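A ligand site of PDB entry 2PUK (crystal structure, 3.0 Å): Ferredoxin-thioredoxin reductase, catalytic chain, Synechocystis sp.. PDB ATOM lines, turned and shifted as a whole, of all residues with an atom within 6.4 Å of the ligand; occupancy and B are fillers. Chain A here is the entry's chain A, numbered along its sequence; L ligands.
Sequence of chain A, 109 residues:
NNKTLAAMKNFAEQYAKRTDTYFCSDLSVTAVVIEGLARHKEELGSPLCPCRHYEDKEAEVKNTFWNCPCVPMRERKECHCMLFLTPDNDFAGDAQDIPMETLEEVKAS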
ATOM      1  N   PHE A  11      24.257  -5.246 -10.628  1.00  0.00           N
ATOM      2  CA  PHE A  11      23.061  -5.879 -10.101  1.00  0.00           C
ATOM      3  C   PHE A  11      22.316  -6.606 -11.206  1.00  0.00           C
ATOM      4  O   PHE A  11      21.908  -7.758 -11.033  1.00  0.00           O
ATOM      5  CB  PHE A  11      22.174  -4.838  -9.405  1.00  0.00           C
ATOM      6  CG  PHE A  11      20.725  -5.198  -9.392  1.00  0.00           C
ATOM      7  CD1 PHE A  11      20.222  -6.099  -8.464  1.00  0.00           C
ATOM      8  CD2 PHE A  11      19.854  -4.644 -10.338  1.00  0.00           C
ATOM      9  CE1 PHE A  11      18.882  -6.438  -8.466  1.00  0.00           C
ATOM     10  CE2 PHE A  11      18.510  -4.980 -10.353  1.00  0.00           C
ATOM     11  CZ  PHE A  11      18.019  -5.878  -9.412  1.00  0.00           C
ATOM     12  N   TYR A  15      22.020 -10.518 -11.068  1.00  0.00           N
ATOM     13  CA  TYR A  15      20.646 -10.970 -10.855  1.00  0.00           C
ATOM     14  C   TYR A  15      20.128 -11.807 -12.030  1.00  0.00           C
ATOM     15  O   TYR A  15      19.438 -12.813 -11.818  1.00  0.00           O
ATOM     16  CB  TYR A  15      19.698  -9.798 -10.555  1.00  0.00           C
ATOM     17  CG  TYR A  15      18.276 -10.204 -10.217  1.00  0.00           C
ATOM     18  CD1 TYR A  15      17.955 -10.653  -8.931  1.00  0.00           C
ATOM     19  CD2 TYR A  15      17.259 -10.138 -11.165  1.00  0.00           C
ATOM     20  CE1 TYR A  15      16.652 -11.037  -8.618  1.00  0.00           C
ATOM     21  CE2 TYR A  15      15.959 -10.526 -10.861  1.00  0.00           C
ATOM     22  CZ  TYR A  15      15.668 -10.968  -9.581  1.00  0.00           C
ATOM     23  OH  TYR A  15      14.374 -11.346  -9.269  1.00  0.00           O
ATOM     24  N   VAL A  33      17.052   0.877 -19.735  1.00  0.00           N
ATOM     25  CA  VAL A  33      16.462   0.482 -18.456  1.00  0.00           C
ATOM     26  C   VAL A  33      17.449   0.681 -17.299  1.00  0.00           C
ATOM     27  O   VAL A  33      17.153   1.403 -16.343  1.00  0.00           O
ATOM     28  CB  VAL A  33      15.958  -0.980 -18.469  1.00  0.00           C
ATOM     29  CG1 VAL A  33      15.352  -1.346 -17.127  1.00  0.00           C
ATOM     30  CG2 VAL A  33      14.959  -1.192 -19.588  1.00  0.00           C
ATOM     31  N   LEU A  37      16.929   2.989 -14.068  1.00  0.00           N
ATOM     32  CA  LEU A  37      16.978   2.476 -12.700  1.00  0.00           C
ATOM     33  C   LEU A  37      17.984   3.257 -11.870  1.00  0.00           C
ATOM     34  O   LEU A  37      17.727   3.572 -10.700  1.00  0.00           O
ATOM     35  CB  LEU A  37      17.331   0.980 -12.698  1.00  0.00           C
ATOM     36  CG  LEU A  37      16.260  -0.007 -13.176  1.00  0.00           C
ATOM     37  CD1 LEU A  37      16.872  -1.324 -13.542  1.00  0.00           C
ATOM     38  CD2 LEU A  37      15.203  -0.207 -12.100  1.00  0.00           C
ATOM     39  N   PRO A  47      15.882   1.842  -6.566  1.00  0.00           N
ATOM     40  CA  PRO A  47      15.877   1.772  -8.023  1.00  0.00           C
ATOM     41  C   PRO A  47      14.475   1.516  -8.557  1.00  0.00           C
ATOM     42  O   PRO A  47      14.160   0.401  -8.992  1.00  0.00           O
ATOM     43  CB  PRO A  47      16.806   0.592  -8.313  1.00  0.00           C
ATOM     44  CG  PRO A  47      16.640  -0.310  -7.148  1.00  0.00           C
ATOM     45  CD  PRO A  47      16.292   0.561  -5.957  1.00  0.00           C
ATOM     46  N   LEU A  48      13.636   2.548  -8.504  1.00  0.00           N
ATOM     47  CA  LEU A  48      12.230   2.451  -8.865  1.00  0.00           C
ATOM     48  C   LEU A  48      12.079   2.219 -10.364  1.00  0.00           C
ATOM     49  O   LEU A  48      12.709   2.902 -11.166  1.00  0.00           O
ATOM     50  CB  LEU A  48      11.505   3.740  -8.470  1.00  0.00           C
ATOM     51  CG  LEU A  48      10.114   3.725  -7.854  1.00  0.00           C
ATOM     52  CD1 LEU A  48       9.422   5.032  -8.175  1.00  0.00           C
ATOM     53  CD2 LEU A  48       9.245   2.572  -8.325  1.00  0.00           C
ATOM     54  N   CYS A  49      11.241   1.239 -10.726  1.00  0.00           N
ATOM     55  CA  CYS A  49      11.048   0.827 -12.118  1.00  0.00           C
ATOM     56  C   CYS A  49      10.817   1.996 -13.081  1.00  0.00           C
ATOM     57  O   CYS A  49       9.933   2.808 -12.868  1.00  0.00           O
ATOM     58  CB  CYS A  49       9.895  -0.172 -12.237  1.00  0.00           C
ATOM     59  SG  CYS A  49       9.843  -1.028 -13.825  1.00  0.00           S
ATOM     60  N   PRO A  50      11.624   2.062 -14.160  1.00  0.00           N
ATOM     61  CA  PRO A  50      11.588   3.195 -15.067  1.00  0.00           C
ATOM     62  C   PRO A  50      10.560   3.023 -16.179  1.00  0.00           C
ATOM     63  O   PRO A  50      10.469   3.869 -17.056  1.00  0.00           O
ATOM     64  CB  PRO A  50      12.986   3.204 -15.656  1.00  0.00           C
ATOM     65  CG  PRO A  50      13.366   1.766 -15.708  1.00  0.00           C
ATOM     66  CD  PRO A  50      12.638   1.071 -14.574  1.00  0.00           C
ATOM     67  N   CYS A  51       9.812   1.923 -16.143  1.00  0.00           N
ATOM     68  CA  CYS A  51       8.774   1.679 -17.133  1.00  0.00           C
ATOM     69  C   CYS A  51       7.365   1.701 -16.550  1.00  0.00           C
ATOM     70  O   CYS A  51       6.525   0.888 -16.923  1.00  0.00           O
ATOM     71  CB  CYS A  51       9.039   0.389 -17.898  1.00  0.00           C
ATOM     72  SG  CYS A  51      10.325   0.582 -19.149  1.00  0.00           S
ATOM     73  N   TRP A  66       7.188  -1.632  -6.640  1.00  0.00           N
ATOM     74  CA  TRP A  66       7.892  -1.470  -7.905  1.00  0.00           C
ATOM     75  C   TRP A  66       9.399  -1.186  -7.776  1.00  0.00           C
ATOM     76  O   TRP A  66      10.027  -0.718  -8.717  1.00  0.00           O
ATOM     77  CB  TRP A  66       7.205  -0.421  -8.796  1.00  0.00           C
ATOM     78  CG  TRP A  66       5.827  -0.848  -9.244  1.00  0.00           C
ATOM     79  CD1 TRP A  66       4.632  -0.392  -8.775  1.00  0.00           C
ATOM     80  CD2 TRP A  66       5.518  -1.825 -10.253  1.00  0.00           C
ATOM     81  NE1 TRP A  66       3.600  -1.019  -9.435  1.00  0.00           N
ATOM     82  CE2 TRP A  66       4.113  -1.906 -10.336  1.00  0.00           C
ATOM     83  CE3 TRP A  66       6.296  -2.638 -11.085  1.00  0.00           C
ATOM     84  CZ2 TRP A  66       3.460  -2.763 -11.230  1.00  0.00           C
ATOM     85  CZ3 TRP A  66       5.643  -3.495 -11.979  1.00  0.00           C
ATOM     86  CH2 TRP A  66       4.247  -3.552 -12.037  1.00  0.00           C
ATOM     87  N   ASN A  67       9.960  -1.502  -6.604  1.00  0.00           N
ATOM     88  CA  ASN A  67      11.410  -1.433  -6.400  1.00  0.00           C
ATOM     89  C   ASN A  67      12.127  -2.650  -6.979  1.00  0.00           C
ATOM     90  O   ASN A  67      11.921  -3.786  -6.533  1.00  0.00           O
ATOM     91  CB  ASN A  67      11.743  -1.277  -4.909  1.00  0.00           C
ATOM     92  CG  ASN A  67      11.477   0.134  -4.393  1.00  0.00           C
ATOM     93  OD1 ASN A  67      11.183   1.042  -5.171  1.00  0.00           O
ATOM     94  ND2 ASN A  67      11.571   0.317  -3.090  1.00  0.00           N
ATOM     95  N   CYS A  68      12.971  -2.407  -7.973  1.00  0.00           N
ATOM     96  CA  CYS A  68      13.646  -3.458  -8.731  1.00  0.00           C
ATOM     97  C   CYS A  68      14.672  -4.247  -7.906  1.00  0.00           C
ATOM     98  O   CYS A  68      15.573  -3.655  -7.310  1.00  0.00           O
ATOM     99  CB  CYS A  68      14.328  -2.862  -9.956  1.00  0.00           C
ATOM    100  SG  CYS A  68      14.963  -4.087 -11.087  1.00  0.00           S
ATOM    101  N   PRO A  69      14.549  -5.592  -7.863  1.00  0.00           N
ATOM    102  CA  PRO A  69      13.532  -6.376  -8.558  1.00  0.00           C
ATOM    103  C   PRO A  69      12.162  -6.293  -7.868  1.00  0.00           C
ATOM    104  O   PRO A  69      12.039  -6.532  -6.663  1.00  0.00           O
ATOM    105  CB  PRO A  69      14.092  -7.809  -8.519  1.00  0.00           C
ATOM    106  CG  PRO A  69      15.428  -7.716  -7.846  1.00  0.00           C
ATOM    107  CD  PRO A  69      15.434  -6.450  -7.077  1.00  0.00           C
ATOM    108  N   CYS A  70      11.165  -5.920  -8.672  1.00  0.00           N
ATOM    109  CA  CYS A  70       9.788  -5.727  -8.240  1.00  0.00           C
ATOM    110  C   CYS A  70       9.120  -7.036  -7.812  1.00  0.00           C
ATOM    111  O   CYS A  70       9.681  -8.116  -8.008  1.00  0.00           O
ATOM    112  CB  CYS A  70       8.994  -5.099  -9.383  1.00  0.00           C
ATOM    113  SG  CYS A  70       9.211  -5.958 -10.955  1.00  0.00           S
ATOM    114  N   VAL A  71       7.921  -6.928  -7.248  1.00  0.00           N
ATOM    115  CA  VAL A  71       7.148  -8.103  -6.865  1.00  0.00           C
ATOM    116  C   VAL A  71       6.851  -9.021  -8.080  1.00  0.00           C
ATOM    117  O   VAL A  71       7.151 -10.207  -8.011  1.00  0.00           O
ATOM    118  CB  VAL A  71       5.866  -7.725  -6.064  1.00  0.00           C
ATOM    119  CG1 VAL A  71       4.787  -8.791  -6.200  1.00  0.00           C
ATOM    120  CG2 VAL A  71       6.219  -7.498  -4.600  1.00  0.00           C
ATOM    121  N   PRO A  72       6.298  -8.473  -9.178  1.00  0.00           N
ATOM    122  CA  PRO A  72       6.023  -9.360 -10.311  1.00  0.00           C
ATOM    123  C   PRO A  72       7.244 -10.150 -10.786  1.00  0.00           C
ATOM    124  O   PRO A  72       7.124 -11.351 -11.026  1.00  0.00           O
ATOM    125  CB  PRO A  72       5.536  -8.401 -11.403  1.00  0.00           C
ATOM    126  CG  PRO A  72       4.948  -7.266 -10.649  1.00  0.00           C
ATOM    127  CD  PRO A  72       5.856  -7.093  -9.456  1.00  0.00           C
ATOM    128  N   MET A  73       8.404  -9.502 -10.886  1.00  0.00           N
ATOM    129  CA  MET A  73       9.617 -10.180 -11.338  1.00  0.00           C
ATOM    130  C   MET A  73      10.159 -11.208 -10.347  1.00  0.00           C
ATOM    131  O   MET A  73      10.746 -12.213 -10.741  1.00  0.00           O
ATOM    132  CB  MET A  73      10.707  -9.173 -11.705  1.00  0.00           C
ATOM    133  CG  MET A  73      12.066  -9.798 -12.062  1.00  0.00           C
ATOM    134  SD  MET A  73      12.035 -10.849 -13.531  1.00  0.00           S
ATOM    135  CE  MET A  73      13.564 -11.747 -13.317  1.00  0.00           C
ATOM    136  N   ARG A  74       9.950 -10.975  -9.057  1.00  0.00           N
ATOM    137  CA  ARG A  74      10.471 -11.870  -8.020  1.00  0.00           C
ATOM    138  C   ARG A  74       9.603 -13.108  -7.826  1.00  0.00           C
ATOM    139  O   ARG A  74      10.131 -14.186  -7.531  1.00  0.00           O
ATOM    140  CB  ARG A  74      10.641 -11.135  -6.685  1.00  0.00           C
ATOM    141  CG  ARG A  74      11.899 -10.277  -6.596  1.00  0.00           C
ATOM    142  CD  ARG A  74      12.134  -9.720  -5.194  1.00  0.00           C
ATOM    143  NE  ARG A  74      11.197  -8.657  -4.852  1.00  0.00           N
ATOM    144  CZ  ARG A  74      10.380  -8.681  -3.806  1.00  0.00           C
ATOM    145  NH1 ARG A  74      10.380  -9.710  -2.981  1.00  0.00           N
ATOM    146  NH2 ARG A  74       9.562  -7.654  -3.574  1.00  0.00           N
ATOM    147  N   GLU A  78       8.010 -11.836 -14.279  1.00  0.00           N
ATOM    148  CA  GLU A  78       7.461 -11.025 -15.363  1.00  0.00           C
ATOM    149  C   GLU A  78       8.049  -9.632 -15.272  1.00  0.00           C
ATOM    150  O   GLU A  78       7.755  -8.896 -14.321  1.00  0.00           O
ATOM    151  CB  GLU A  78       5.926 -10.981 -15.278  1.00  0.00           C
ATOM    152  CG  GLU A  78       5.293 -12.358 -15.036  1.00  0.00           C
ATOM    153  CD  GLU A  78       3.777 -12.331 -14.893  1.00  0.00           C
ATOM    154  OE1 GLU A  78       3.194 -11.285 -14.529  1.00  0.00           O
ATOM    155  OE2 GLU A  78       3.170 -13.402 -15.129  1.00  0.00           O
ATOM    156  N   CYS A  79       8.891  -9.282 -16.237  1.00  0.00           N
ATOM    157  CA  CYS A  79       9.601  -8.013 -16.260  1.00  0.00           C
ATOM    158  C   CYS A  79       9.255  -7.228 -17.517  1.00  0.00           C
ATOM    159  O   CYS A  79       9.711  -7.564 -18.613  1.00  0.00           O
ATOM    160  CB  CYS A  79      11.107  -8.247 -16.161  1.00  0.00           C
ATOM    161  SG  CYS A  79      12.093  -6.785 -16.509  1.00  0.00           S
ATOM    162  N   HIS A  80       8.471  -6.173 -17.369  1.00  0.00           N
ATOM    163  CA  HIS A  80       7.937  -5.459 -18.528  1.00  0.00           C
ATOM    164  C   HIS A  80       8.852  -4.379 -19.113  1.00  0.00           C
ATOM    165  O   HIS A  80       8.582  -3.873 -20.206  1.00  0.00           O
ATOM    166  CB  HIS A  80       6.519  -4.949 -18.268  1.00  0.00           C
ATOM    167  CG  HIS A  80       6.415  -4.007 -17.114  1.00  0.00           C
ATOM    168  ND1 HIS A  80       6.420  -2.636 -17.258  1.00  0.00           N
ATOM    169  CD2 HIS A  80       6.297  -4.237 -15.775  1.00  0.00           C
ATOM    170  CE1 HIS A  80       6.314  -2.070 -16.075  1.00  0.00           C
ATOM    171  NE2 HIS A  80       6.240  -3.024 -15.157  1.00  0.00           N
ATOM    172  N   CYS A  81       9.918  -4.023 -18.396  1.00  0.00           N
ATOM    173  CA  CYS A  81      10.965  -3.167 -18.976  1.00  0.00           C
ATOM    174  C   CYS A  81      11.790  -3.978 -19.967  1.00  0.00           C
ATOM    175  O   CYS A  81      12.563  -3.417 -20.754  1.00  0.00           O
ATOM    176  CB  CYS A  81      11.917  -2.650 -17.911  1.00  0.00           C
ATOM    177  SG  CYS A  81      11.172  -1.784 -16.550  1.00  0.00           S
ATOM    178  N   MET A  82      11.636  -5.296 -19.910  1.00  0.00           N
ATOM    179  CA  MET A  82      12.430  -6.242 -20.699  1.00  0.00           C
ATOM    180  C   MET A  82      13.915  -6.118 -20.352  1.00  0.00           C
ATOM    181  O   MET A  82      14.787  -6.064 -21.227  1.00  0.00           O
ATOM    182  CB  MET A  82      12.172  -6.066 -22.202  1.00  0.00           C
ATOM    183  CG  MET A  82      10.789  -6.502 -22.635  1.00  0.00           C
ATOM    184  SD  MET A  82      10.306  -5.718 -24.178  1.00  0.00           S
ATOM    185  CE  MET A  82      11.538  -6.337 -25.311  1.00  0.00           C
ATOM    186  N   LEU A  83      14.181  -6.047 -19.054  1.00  0.00           N
ATOM    187  CA  LEU A  83      15.528  -6.203 -18.544  1.00  0.00           C
ATOM    188  C   LEU A  83      15.762  -7.689 -18.385  1.00  0.00           C
ATOM    189  O   LEU A  83      16.659  -8.253 -19.019  1.00  0.00           O
ATOM    190  CB  LEU A  83      15.674  -5.486 -17.207  1.00  0.00           C
ATOM    191  CG  LEU A  83      17.089  -5.110 -16.771  1.00  0.00           C
ATOM    192  CD1 LEU A  83      17.756  -4.222 -17.808  1.00  0.00           C
ATOM    193  CD2 LEU A  83      17.046  -4.407 -15.420  1.00  0.00           C
ATOM    194  N   PHE A  84      14.932  -8.338 -17.572  1.00  0.00           N
ATOM    195  CA  PHE A  84      15.065  -9.762 -17.310  1.00  0.00           C
ATOM    196  C   PHE A  84      14.077 -10.596 -18.111  1.00  0.00           C
ATOM    197  O   PHE A  84      12.940 -10.822 -17.702  1.00  0.00           O
ATOM    198  CB  PHE A  84      14.931 -10.049 -15.801  1.00  0.00           C
ATOM    199  CG  PHE A  84      15.663  -9.065 -14.922  1.00  0.00           C
ATOM    200  CD1 PHE A  84      14.957  -8.127 -14.187  1.00  0.00           C
ATOM    201  CD2 PHE A  84      17.055  -9.084 -14.841  1.00  0.00           C
ATOM    202  CE1 PHE A  84      15.622  -7.213 -13.373  1.00  0.00           C
ATOM    203  CE2 PHE A  84      17.722  -8.173 -14.036  1.00  0.00           C
ATOM    204  CZ  PHE A  84      17.003  -7.234 -13.304  1.00  0.00           C
HETATM  205 FE1  LIG L   1      10.505  -5.043 -12.464  1.00  0.00          FE
HETATM  206 FE2  LIG L   1      11.758  -5.432 -14.632  1.00  0.00          FE
HETATM  207 FE3  LIG L   1      12.934  -4.389 -12.664  1.00  0.00          FE
HETATM  208 FE4  LIG L   1      11.165  -3.083 -13.917  1.00  0.00          FE
HETATM  209  S1  LIG L   1      13.031  -3.764 -14.682  1.00  0.00           S
HETATM  210  S2  LIG L   1      11.379  -3.244 -11.807  1.00  0.00           S
HETATM  211  S3  LIG L   1       9.819  -4.623 -14.423  1.00  0.00           S
HETATM  212  S4  LIG L   1      12.140  -6.344 -12.771  1.00  0.00           S
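SG of Cys 70 is bound to FE1 of the ligand, 2.2 Å away.
The side-chain sulfur (SG) of Cys 49 is bound to an iron atom (FE4) of the ligand, 2.4 Å away.
The backbone NH of His 80 sits close to a sulfur (S3) of the ligand (3.6 Å).
An iron atom (FE3) of the ligand is bound by the side-chain sulfur (SG) of Cys 68 (2.6 Å).
SG of Cys 81 lies close to S1 of the ligand, 3.3 Å away.
SG of Cys 79 binds FE2 of the ligand (2.3 Å).
Merely in contact with the ligand: Met 73 (3.3 Å) and Phe 84 (3.6 Å).
Hydrophobic or aromatic side chains within 4 Å of the ligand: Met 73, His 80 and Phe 84.
Of the 25 residues printed, 8 come within 4 Å of the ligand.
The side-chain sulfur of Cys 81 sits close to the side-chain sulfur of Cys 51, at 3.6 Å.
The side-chain sulfur of Cys 49 sits close to the backbone NH of Cys 51 (3.8 Å).
The backbone carbonyl oxygen (O) of Trp 66 sits at hydrogen-bond distance from the backbone NH (N) of Cys 49 (3.1 Å).
SG of Cys 79 sits close to N of Leu 83 (3.4 Å).
SG of Cys 79 lies close to N of Phe 84, 3.4 Å away.
The backbone NH (N) of Cys 68 sits at hydrogen-bond distance from the backbone carbonyl oxygen (O) of Pro 47.
The backbone NH (N) of Met 73 sits close to the side-chain sulfur (SG) of Cys 70 (3.6 Å).
The side-chain sulfur (SG) of Cys 49 lies close to the side-chain sulfur (SG) of Cys 81, 3.1 Å away.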
